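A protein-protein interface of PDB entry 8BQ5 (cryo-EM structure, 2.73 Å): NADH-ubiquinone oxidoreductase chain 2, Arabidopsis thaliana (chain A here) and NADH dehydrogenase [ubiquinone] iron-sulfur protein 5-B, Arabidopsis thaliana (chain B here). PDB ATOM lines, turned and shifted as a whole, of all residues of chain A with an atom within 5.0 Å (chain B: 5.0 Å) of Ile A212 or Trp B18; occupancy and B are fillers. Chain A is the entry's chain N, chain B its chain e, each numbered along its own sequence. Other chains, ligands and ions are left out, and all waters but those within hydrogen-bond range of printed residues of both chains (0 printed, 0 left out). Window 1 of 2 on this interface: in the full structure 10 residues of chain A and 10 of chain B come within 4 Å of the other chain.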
ATOM      1  N   THR A 201     -12.098 -16.382 -13.882  1.00  0.00           N
ATOM      2  CA  THR A 201     -10.734 -16.776 -14.219  1.00  0.00           C
ATOM      3  C   THR A 201     -10.376 -16.616 -15.690  1.00  0.00           C
ATOM      4  O   THR A 201      -9.188 -16.668 -16.025  1.00  0.00           O
ATOM      5  CB  THR A 201     -10.480 -18.234 -13.808  1.00  0.00           C
ATOM      6  OG1 THR A 201     -11.144 -19.114 -14.723  1.00  0.00           O
ATOM      7  CG2 THR A 201     -10.988 -18.491 -12.400  1.00  0.00           C
ATOM      8  N   ALA A 203     -10.908 -18.798 -17.976  1.00  0.00           N
ATOM      9  CA  ALA A 203     -10.418 -20.096 -18.409  1.00  0.00           C
ATOM     10  C   ALA A 203     -11.491 -21.154 -18.194  1.00  0.00           C
ATOM     11  O   ALA A 203     -12.327 -21.037 -17.294  1.00  0.00           O
ATOM     12  CB  ALA A 203      -9.140 -20.489 -17.656  1.00  0.00           C
ATOM     13  N   GLN A 208      -5.534 -24.965 -16.975  1.00  0.00           N
ATOM     14  CA  GLN A 208      -5.525 -23.537 -16.682  1.00  0.00           C
ATOM     15  C   GLN A 208      -6.192 -23.256 -15.344  1.00  0.00           C
ATOM     16  O   GLN A 208      -5.709 -22.430 -14.561  1.00  0.00           O
ATOM     17  CB  GLN A 208      -6.219 -22.760 -17.801  1.00  0.00           C
ATOM     18  CG  GLN A 208      -5.728 -23.084 -19.204  1.00  0.00           C
ATOM     19  CD  GLN A 208      -6.668 -22.568 -20.278  1.00  0.00           C
ATOM     20  OE1 GLN A 208      -7.855 -22.359 -20.031  1.00  0.00           O
ATOM     21  NE2 GLN A 208      -6.138 -22.349 -21.475  1.00  0.00           N
ATOM     22  N   LEU A 209      -7.301 -23.941 -15.063  1.00  0.00           N
ATOM     23  CA  LEU A 209      -7.960 -23.797 -13.769  1.00  0.00           C
ATOM     24  C   LEU A 209      -7.069 -24.287 -12.637  1.00  0.00           C
ATOM     25  O   LEU A 209      -7.051 -23.698 -11.551  1.00  0.00           O
ATOM     26  CB  LEU A 209      -9.287 -24.553 -13.774  1.00  0.00           C
ATOM     27  CG  LEU A 209     -10.408 -23.940 -14.613  1.00  0.00           C
ATOM     28  CD1 LEU A 209     -11.760 -24.459 -14.156  1.00  0.00           C
ATOM     29  CD2 LEU A 209     -10.360 -22.427 -14.512  1.00  0.00           C
ATOM     30  N   ALA A 210      -6.327 -25.372 -12.867  1.00  0.00           N
ATOM     31  CA  ALA A 210      -5.434 -25.887 -11.836  1.00  0.00           C
ATOM     32  C   ALA A 210      -4.354 -24.869 -11.493  1.00  0.00           C
ATOM     33  O   ALA A 210      -4.045 -24.649 -10.318  1.00  0.00           O
ATOM     34  CB  ALA A 210      -4.813 -27.208 -12.291  1.00  0.00           C
ATOM     35  N   LYS A 211      -3.776 -24.226 -12.511  1.00  0.00           N
ATOM     36  CA  LYS A 211      -2.721 -23.249 -12.248  1.00  0.00           C
ATOM     37  C   LYS A 211      -3.256 -22.020 -11.520  1.00  0.00           C
ATOM     38  O   LYS A 211      -2.664 -21.574 -10.529  1.00  0.00           O
ATOM     39  CB  LYS A 211      -2.049 -22.828 -13.552  1.00  0.00           C
ATOM     40  CG  LYS A 211      -0.983 -23.774 -14.054  1.00  0.00           C
ATOM     41  CD  LYS A 211      -0.645 -23.440 -15.492  1.00  0.00           C
ATOM     42  CE  LYS A 211       0.653 -24.083 -15.929  1.00  0.00           C
ATOM     43  NZ  LYS A 211       0.550 -25.564 -15.913  1.00  0.00           N
ATOM     44  N   ILE A 212      -4.369 -21.457 -11.994  1.00  0.00           N
ATOM     45  CA  ILE A 212      -4.882 -20.212 -11.426  1.00  0.00           C
ATOM     46  C   ILE A 212      -5.270 -20.405  -9.965  1.00  0.00           C
ATOM     47  O   ILE A 212      -4.995 -19.548  -9.115  1.00  0.00           O
ATOM     48  CB  ILE A 212      -6.070 -19.684 -12.253  1.00  0.00           C
ATOM     49  CG1 ILE A 212      -5.590 -19.093 -13.575  1.00  0.00           C
ATOM     50  CG2 ILE A 212      -6.849 -18.632 -11.478  1.00  0.00           C
ATOM     51  CD1 ILE A 212      -6.602 -19.204 -14.695  1.00  0.00           C
ATOM     52  N   LEU A 213      -5.907 -21.531  -9.647  1.00  0.00           N
ATOM     53  CA  LEU A 213      -6.456 -21.710  -8.270  1.00  0.00           C
ATOM     54  C   LEU A 213      -5.395 -22.154  -7.267  1.00  0.00           C
ATOM     55  O   LEU A 213      -5.559 -21.819  -6.085  1.00  0.00           O
ATOM     56  CB  LEU A 213      -7.581 -22.748  -8.319  1.00  0.00           C
ATOM     57  CG  LEU A 213      -8.798 -22.380  -9.166  1.00  0.00           C
ATOM     58  CD1 LEU A 213      -9.972 -23.284  -8.829  1.00  0.00           C
ATOM     59  CD2 LEU A 213      -9.178 -20.923  -8.965  1.00  0.00           C
ATOM     60  N   THR A 214      -4.360 -22.871  -7.709  1.00  0.00           N
ATOM     61  CA  THR A 214      -3.375 -23.434  -6.747  1.00  0.00           C
ATOM     62  C   THR A 214      -2.627 -22.369  -5.964  1.00  0.00           C
ATOM     63  O   THR A 214      -2.235 -21.361  -6.568  1.00  0.00           O
ATOM     64  CB  THR A 214      -2.272 -24.270  -7.406  1.00  0.00           C
ATOM     65  OG1 THR A 214      -1.866 -23.634  -8.619  1.00  0.00           O
ATOM     66  CG2 THR A 214      -2.697 -25.694  -7.690  1.00  0.00           C
ATOM     67  N   TYR A 216      -3.615 -20.476  -3.272  1.00  0.00           N
ATOM     68  CA  TYR A 216      -4.305 -19.372  -2.614  1.00  0.00           C
ATOM     69  C   TYR A 216      -5.525 -19.805  -1.820  1.00  0.00           C
ATOM     70  O   TYR A 216      -5.737 -19.291  -0.719  1.00  0.00           O
ATOM     71  CB  TYR A 216      -4.706 -18.325  -3.662  1.00  0.00           C
ATOM     72  CG  TYR A 216      -3.513 -17.615  -4.244  1.00  0.00           C
ATOM     73  CD1 TYR A 216      -2.757 -18.204  -5.246  1.00  0.00           C
ATOM     74  CD2 TYR A 216      -3.139 -16.359  -3.789  1.00  0.00           C
ATOM     75  CE1 TYR A 216      -1.661 -17.568  -5.772  1.00  0.00           C
ATOM     76  CE2 TYR A 216      -2.044 -15.710  -4.318  1.00  0.00           C
ATOM     77  CZ  TYR A 216      -1.311 -16.321  -5.310  1.00  0.00           C
ATOM     78  OH  TYR A 216      -0.217 -15.689  -5.846  1.00  0.00           O
ATOM     79  N   ALA B   2      -7.243 -16.675 -21.431  1.00  0.00           N
ATOM     80  CA  ALA B   2      -6.209 -17.702 -21.364  1.00  0.00           C
ATOM     81  C   ALA B   2      -6.083 -18.482 -22.672  1.00  0.00           C
ATOM     82  O   ALA B   2      -5.058 -19.109 -22.924  1.00  0.00           O
ATOM     83  CB  ALA B   2      -6.488 -18.655 -20.210  1.00  0.00           C
ATOM     84  N   CYS B  14      -5.451 -10.274 -22.702  1.00  0.00           N
ATOM     85  CA  CYS B  14      -4.751 -10.733 -21.513  1.00  0.00           C
ATOM     86  C   CYS B  14      -3.948 -12.004 -21.748  1.00  0.00           C
ATOM     87  O   CYS B  14      -3.534 -12.649 -20.781  1.00  0.00           O
ATOM     88  CB  CYS B  14      -5.752 -10.948 -20.380  1.00  0.00           C
ATOM     89  SG  CYS B  14      -6.649  -9.455 -19.938  1.00  0.00           S
ATOM     90  N   TYR B  15      -3.713 -12.375 -23.007  1.00  0.00           N
ATOM     91  CA  TYR B  15      -3.088 -13.662 -23.289  1.00  0.00           C
ATOM     92  C   TYR B  15      -1.612 -13.671 -22.913  1.00  0.00           C
ATOM     93  O   TYR B  15      -1.106 -14.677 -22.412  1.00  0.00           O
ATOM     94  CB  TYR B  15      -3.264 -14.019 -24.762  1.00  0.00           C
ATOM     95  CG  TYR B  15      -2.605 -15.319 -25.148  1.00  0.00           C
ATOM     96  CD1 TYR B  15      -3.050 -16.526 -24.626  1.00  0.00           C
ATOM     97  CD2 TYR B  15      -1.532 -15.340 -26.027  1.00  0.00           C
ATOM     98  CE1 TYR B  15      -2.455 -17.717 -24.978  1.00  0.00           C
ATOM     99  CE2 TYR B  15      -0.929 -16.525 -26.383  1.00  0.00           C
ATOM    100  CZ  TYR B  15      -1.395 -17.711 -25.856  1.00  0.00           C
ATOM    101  OH  TYR B  15      -0.795 -18.896 -26.206  1.00  0.00           O
ATOM    102  N   ASP B  16      -0.899 -12.570 -23.165  1.00  0.00           N
ATOM    103  CA  ASP B  16       0.522 -12.525 -22.832  1.00  0.00           C
ATOM    104  C   ASP B  16       0.744 -12.622 -21.329  1.00  0.00           C
ATOM    105  O   ASP B  16       1.658 -13.317 -20.874  1.00  0.00           O
ATOM    106  CB  ASP B  16       1.149 -11.251 -23.388  1.00  0.00           C
ATOM    107  CG  ASP B  16       1.402 -11.334 -24.874  1.00  0.00           C
ATOM    108  OD1 ASP B  16       1.506 -12.462 -25.395  1.00  0.00           O
ATOM    109  OD2 ASP B  16       1.487 -10.270 -25.522  1.00  0.00           O
ATOM    110  N   PHE B  17      -0.082 -11.934 -20.540  1.00  0.00           N
ATOM    111  CA  PHE B  17       0.007 -12.062 -19.091  1.00  0.00           C
ATOM    112  C   PHE B  17      -0.242 -13.501 -18.661  1.00  0.00           C
ATOM    113  O   PHE B  17       0.468 -14.040 -17.802  1.00  0.00           O
ATOM    114  CB  PHE B  17      -0.998 -11.127 -18.423  1.00  0.00           C
ATOM    115  CG  PHE B  17      -0.596  -9.687 -18.453  1.00  0.00           C
ATOM    116  CD1 PHE B  17       0.523  -9.259 -17.766  1.00  0.00           C
ATOM    117  CD2 PHE B  17      -1.339  -8.759 -19.159  1.00  0.00           C
ATOM    118  CE1 PHE B  17       0.897  -7.936 -17.787  1.00  0.00           C
ATOM    119  CE2 PHE B  17      -0.969  -7.433 -19.181  1.00  0.00           C
ATOM    120  CZ  PHE B  17       0.152  -7.022 -18.496  1.00  0.00           C
ATOM    121  N   TRP B  18      -1.252 -14.137 -19.258  1.00  0.00           N
ATOM    122  CA  TRP B  18      -1.550 -15.524 -18.931  1.00  0.00           C
ATOM    123  C   TRP B  18      -0.374 -16.419 -19.255  1.00  0.00           C
ATOM    124  O   TRP B  18      -0.007 -17.302 -18.469  1.00  0.00           O
ATOM    125  CB  TRP B  18      -2.772 -16.012 -19.701  1.00  0.00           C
ATOM    126  CG  TRP B  18      -2.848 -17.494 -19.659  1.00  0.00           C
ATOM    127  CD1 TRP B  18      -2.629 -18.366 -20.687  1.00  0.00           C
ATOM    128  CD2 TRP B  18      -3.109 -18.292 -18.507  1.00  0.00           C
ATOM    129  NE1 TRP B  18      -2.765 -19.658 -20.245  1.00  0.00           N
ATOM    130  CE2 TRP B  18      -3.059 -19.638 -18.908  1.00  0.00           C
ATOM    131  CE3 TRP B  18      -3.394 -17.994 -17.173  1.00  0.00           C
ATOM    132  CZ2 TRP B  18      -3.285 -20.685 -18.022  1.00  0.00           C
ATOM    133  CZ3 TRP B  18      -3.612 -19.028 -16.302  1.00  0.00           C
ATOM    134  CH2 TRP B  18      -3.562 -20.359 -16.726  1.00  0.00           C
ATOM    135  N   MET B  19       0.212 -16.224 -20.430  1.00  0.00           N
ATOM    136  CA  MET B  19       1.334 -17.062 -20.779  1.00  0.00           C
ATOM    137  C   MET B  19       2.446 -16.861 -19.769  1.00  0.00           C
ATOM    138  O   MET B  19       2.818 -17.822 -19.092  1.00  0.00           O
ATOM    139  CB  MET B  19       1.768 -16.810 -22.223  1.00  0.00           C
ATOM    140  CG  MET B  19       0.840 -17.524 -23.210  1.00  0.00           C
ATOM    141  SD  MET B  19       0.463 -19.226 -22.712  1.00  0.00           S
ATOM    142  CE  MET B  19       1.318 -20.161 -23.976  1.00  0.00           C
ATOM    143  N   ASP B  20       2.878 -15.617 -19.531  1.00  0.00           N
ATOM    144  CA  ASP B  20       3.980 -15.384 -18.594  1.00  0.00           C
ATOM    145  C   ASP B  20       3.712 -16.037 -17.240  1.00  0.00           C
ATOM    146  O   ASP B  20       4.606 -16.659 -16.650  1.00  0.00           O
ATOM    147  CB  ASP B  20       4.229 -13.885 -18.441  1.00  0.00           C
ATOM    148  CG  ASP B  20       4.627 -13.235 -19.744  1.00  0.00           C
ATOM    149  OD1 ASP B  20       4.163 -13.699 -20.804  1.00  0.00           O
ATOM    150  OD2 ASP B  20       5.410 -12.266 -19.718  1.00  0.00           O
ATOM    151  N   PHE B  21       2.471 -15.944 -16.755  1.00  0.00           N
ATOM    152  CA  PHE B  21       2.088 -16.677 -15.551  1.00  0.00           C
ATOM    153  C   PHE B  21       2.329 -18.175 -15.714  1.00  0.00           C
ATOM    154  O   PHE B  21       2.836 -18.838 -14.799  1.00  0.00           O
ATOM    155  CB  PHE B  21       0.618 -16.402 -15.230  1.00  0.00           C
ATOM    156  CG  PHE B  21       0.078 -17.217 -14.092  1.00  0.00           C
ATOM    157  CD1 PHE B  21       0.752 -17.286 -12.886  1.00  0.00           C
ATOM    158  CD2 PHE B  21      -1.103 -17.929 -14.233  1.00  0.00           C
ATOM    159  CE1 PHE B  21       0.253 -18.035 -11.841  1.00  0.00           C
ATOM    160  CE2 PHE B  21      -1.604 -18.683 -13.191  1.00  0.00           C
ATOM    161  CZ  PHE B  21      -0.924 -18.737 -11.995  1.00  0.00           C
ATOM    162  N   SER B  22       1.980 -18.723 -16.883  1.00  0.00           N
ATOM    163  CA  SER B  22       2.067 -20.168 -17.086  1.00  0.00           C
ATOM    164  C   SER B  22       3.517 -20.641 -17.191  1.00  0.00           C
ATOM    165  O   SER B  22       3.883 -21.662 -16.598  1.00  0.00           O
ATOM    166  CB  SER B  22       1.264 -20.565 -18.327  1.00  0.00           C
ATOM    167  OG  SER B  22      -0.118 -20.323 -18.153  1.00  0.00           O
ATOM    168  N   ARG B  38       0.652 -13.641 -11.593  1.00  0.00           N
ATOM    169  CA  ARG B  38      -0.742 -14.045 -11.453  1.00  0.00           C
ATOM    170  C   ARG B  38      -1.645 -12.844 -11.212  1.00  0.00           C
ATOM    171  O   ARG B  38      -2.716 -12.724 -11.825  1.00  0.00           O
ATOM    172  CB  ARG B  38      -0.878 -15.057 -10.317  1.00  0.00           C
ATOM    173  CG  ARG B  38      -2.285 -15.587 -10.118  1.00  0.00           C
ATOM    174  CD  ARG B  38      -2.479 -16.048  -8.689  1.00  0.00           C
ATOM    175  NE  ARG B  38      -3.712 -16.803  -8.499  1.00  0.00           N
ATOM    176  CZ  ARG B  38      -4.761 -16.361  -7.820  1.00  0.00           C
ATOM    177  NH1 ARG B  38      -4.768 -15.161  -7.264  1.00  0.00           N
ATOM    178  NH2 ARG B  38      -5.829 -17.143  -7.694  1.00  0.00           N
ATOM    179  N   TYR B  41      -2.063 -10.915 -14.414  1.00  0.00           N
ATOM    180  CA  TYR B  41      -3.068 -11.502 -15.299  1.00  0.00           C
ATOM    181  C   TYR B  41      -4.482 -11.186 -14.818  1.00  0.00           C
ATOM    182  O   TYR B  41      -5.360 -10.818 -15.612  1.00  0.00           O
ATOM    183  CB  TYR B  41      -2.861 -13.013 -15.404  1.00  0.00           C
ATOM    184  CG  TYR B  41      -4.017 -13.745 -16.048  1.00  0.00           C
ATOM    185  CD1 TYR B  41      -4.282 -13.613 -17.405  1.00  0.00           C
ATOM    186  CD2 TYR B  41      -4.851 -14.560 -15.297  1.00  0.00           C
ATOM    187  CE1 TYR B  41      -5.340 -14.277 -17.995  1.00  0.00           C
ATOM    188  CE2 TYR B  41      -5.909 -15.227 -15.876  1.00  0.00           C
ATOM    189  CZ  TYR B  41      -6.148 -15.083 -17.226  1.00  0.00           C
ATOM    190  OH  TYR B  41      -7.203 -15.747 -17.802  1.00  0.00           O
ATOM    191  N   LEU B  42      -4.723 -11.320 -13.511  1.00  0.00           N
ATOM    192  CA  LEU B  42      -6.051 -11.004 -12.991  1.00  0.00           C
ATOM    193  C   LEU B  42      -6.369  -9.515 -13.110  1.00  0.00           C
ATOM    194  O   LEU B  42      -7.526  -9.144 -13.349  1.00  0.00           O
ATOM    195  CB  LEU B  42      -6.182 -11.475 -11.542  1.00  0.00           C
ATOM    196  CG  LEU B  42      -5.948 -12.970 -11.303  1.00  0.00           C
ATOM    197  CD1 LEU B  42      -6.045 -13.312  -9.825  1.00  0.00           C
ATOM    198  CD2 LEU B  42      -6.931 -13.803 -12.109  1.00  0.00           C
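OH of Tyr B41 lies within hydrogen-bond range of O of Thr A201. The backbone carbonyl oxygen (O) of Ile A212 lies within hydrogen-bond range of the guanidinium group (NH2) of Arg B38 (2.9 Å).
Of the 13 printed residues of chain B, 5 touch a printed residue of chain A. Hydrophobic or aromatic side chains of chain B that line the printed part of chain A: Ala B2, Trp B18, Phe B21 and Tyr B41. Of the 10 printed residues of chain A, 5 touch a printed residue of chain B. Hydrophobic or aromatic side chains of chain A that line the printed part of chain B: Ile A212 and Tyr A216. Along chain A the printed residues that touch a printed residue of chain B span positions 201 to 216. Among the printed residues, no Asp or Glu carboxylate lies within 4 Å of a Lys or Arg side-chain nitrogen of the other chain.
The side-chain hydroxyl of Thr A201 sits close to the backbone NH of Ala A203. The backbone carbonyl oxygen (O) of Trp B18 lies within hydrogen-bond range of the side-chain hydroxyl (OG) of Ser B22 (3.0 Å). The backbone carbonyl oxygen of Lys A211 lies within hydrogen-bond range of the side-chain hydroxyl of Thr A214 (2.9 Å).
Printed residues of chain B within 4 Å of Gln A208: Ala B2 (3.7 Å) and Trp B18 (3.6 Å). Asp B16 touches none of the printed residues of chain A. Of chain A, only Gln A208 and Ile A212 come within 4 Å of Trp B18. Printed residues of chain A within 4 Å of Tyr B41: Thr A201. The nearest residue of chain B that does not touch Ile A212 is Phe B21 (4.02 Å). The nearest residue of chain A that does not touch Trp B18 is Lys A211 (4.3 Å). The nearest printed residue of chain A that does not touch Phe B21 is Ile A212 (4.02 Å).
Gln A208 touches Ala B2 (NE2 to O, 3.7 Å). CB of Gln A208 touches CZ2 of Trp B18, 3.6 Å away. Lys A211 touches Phe B21 (O to CZ, 3.6 Å). CG1 of Ile A212 touches CZ3 of Trp B18 (3.4 Å). CE1 of Tyr A216 touches CD of Arg B38, 3.4 Å away.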
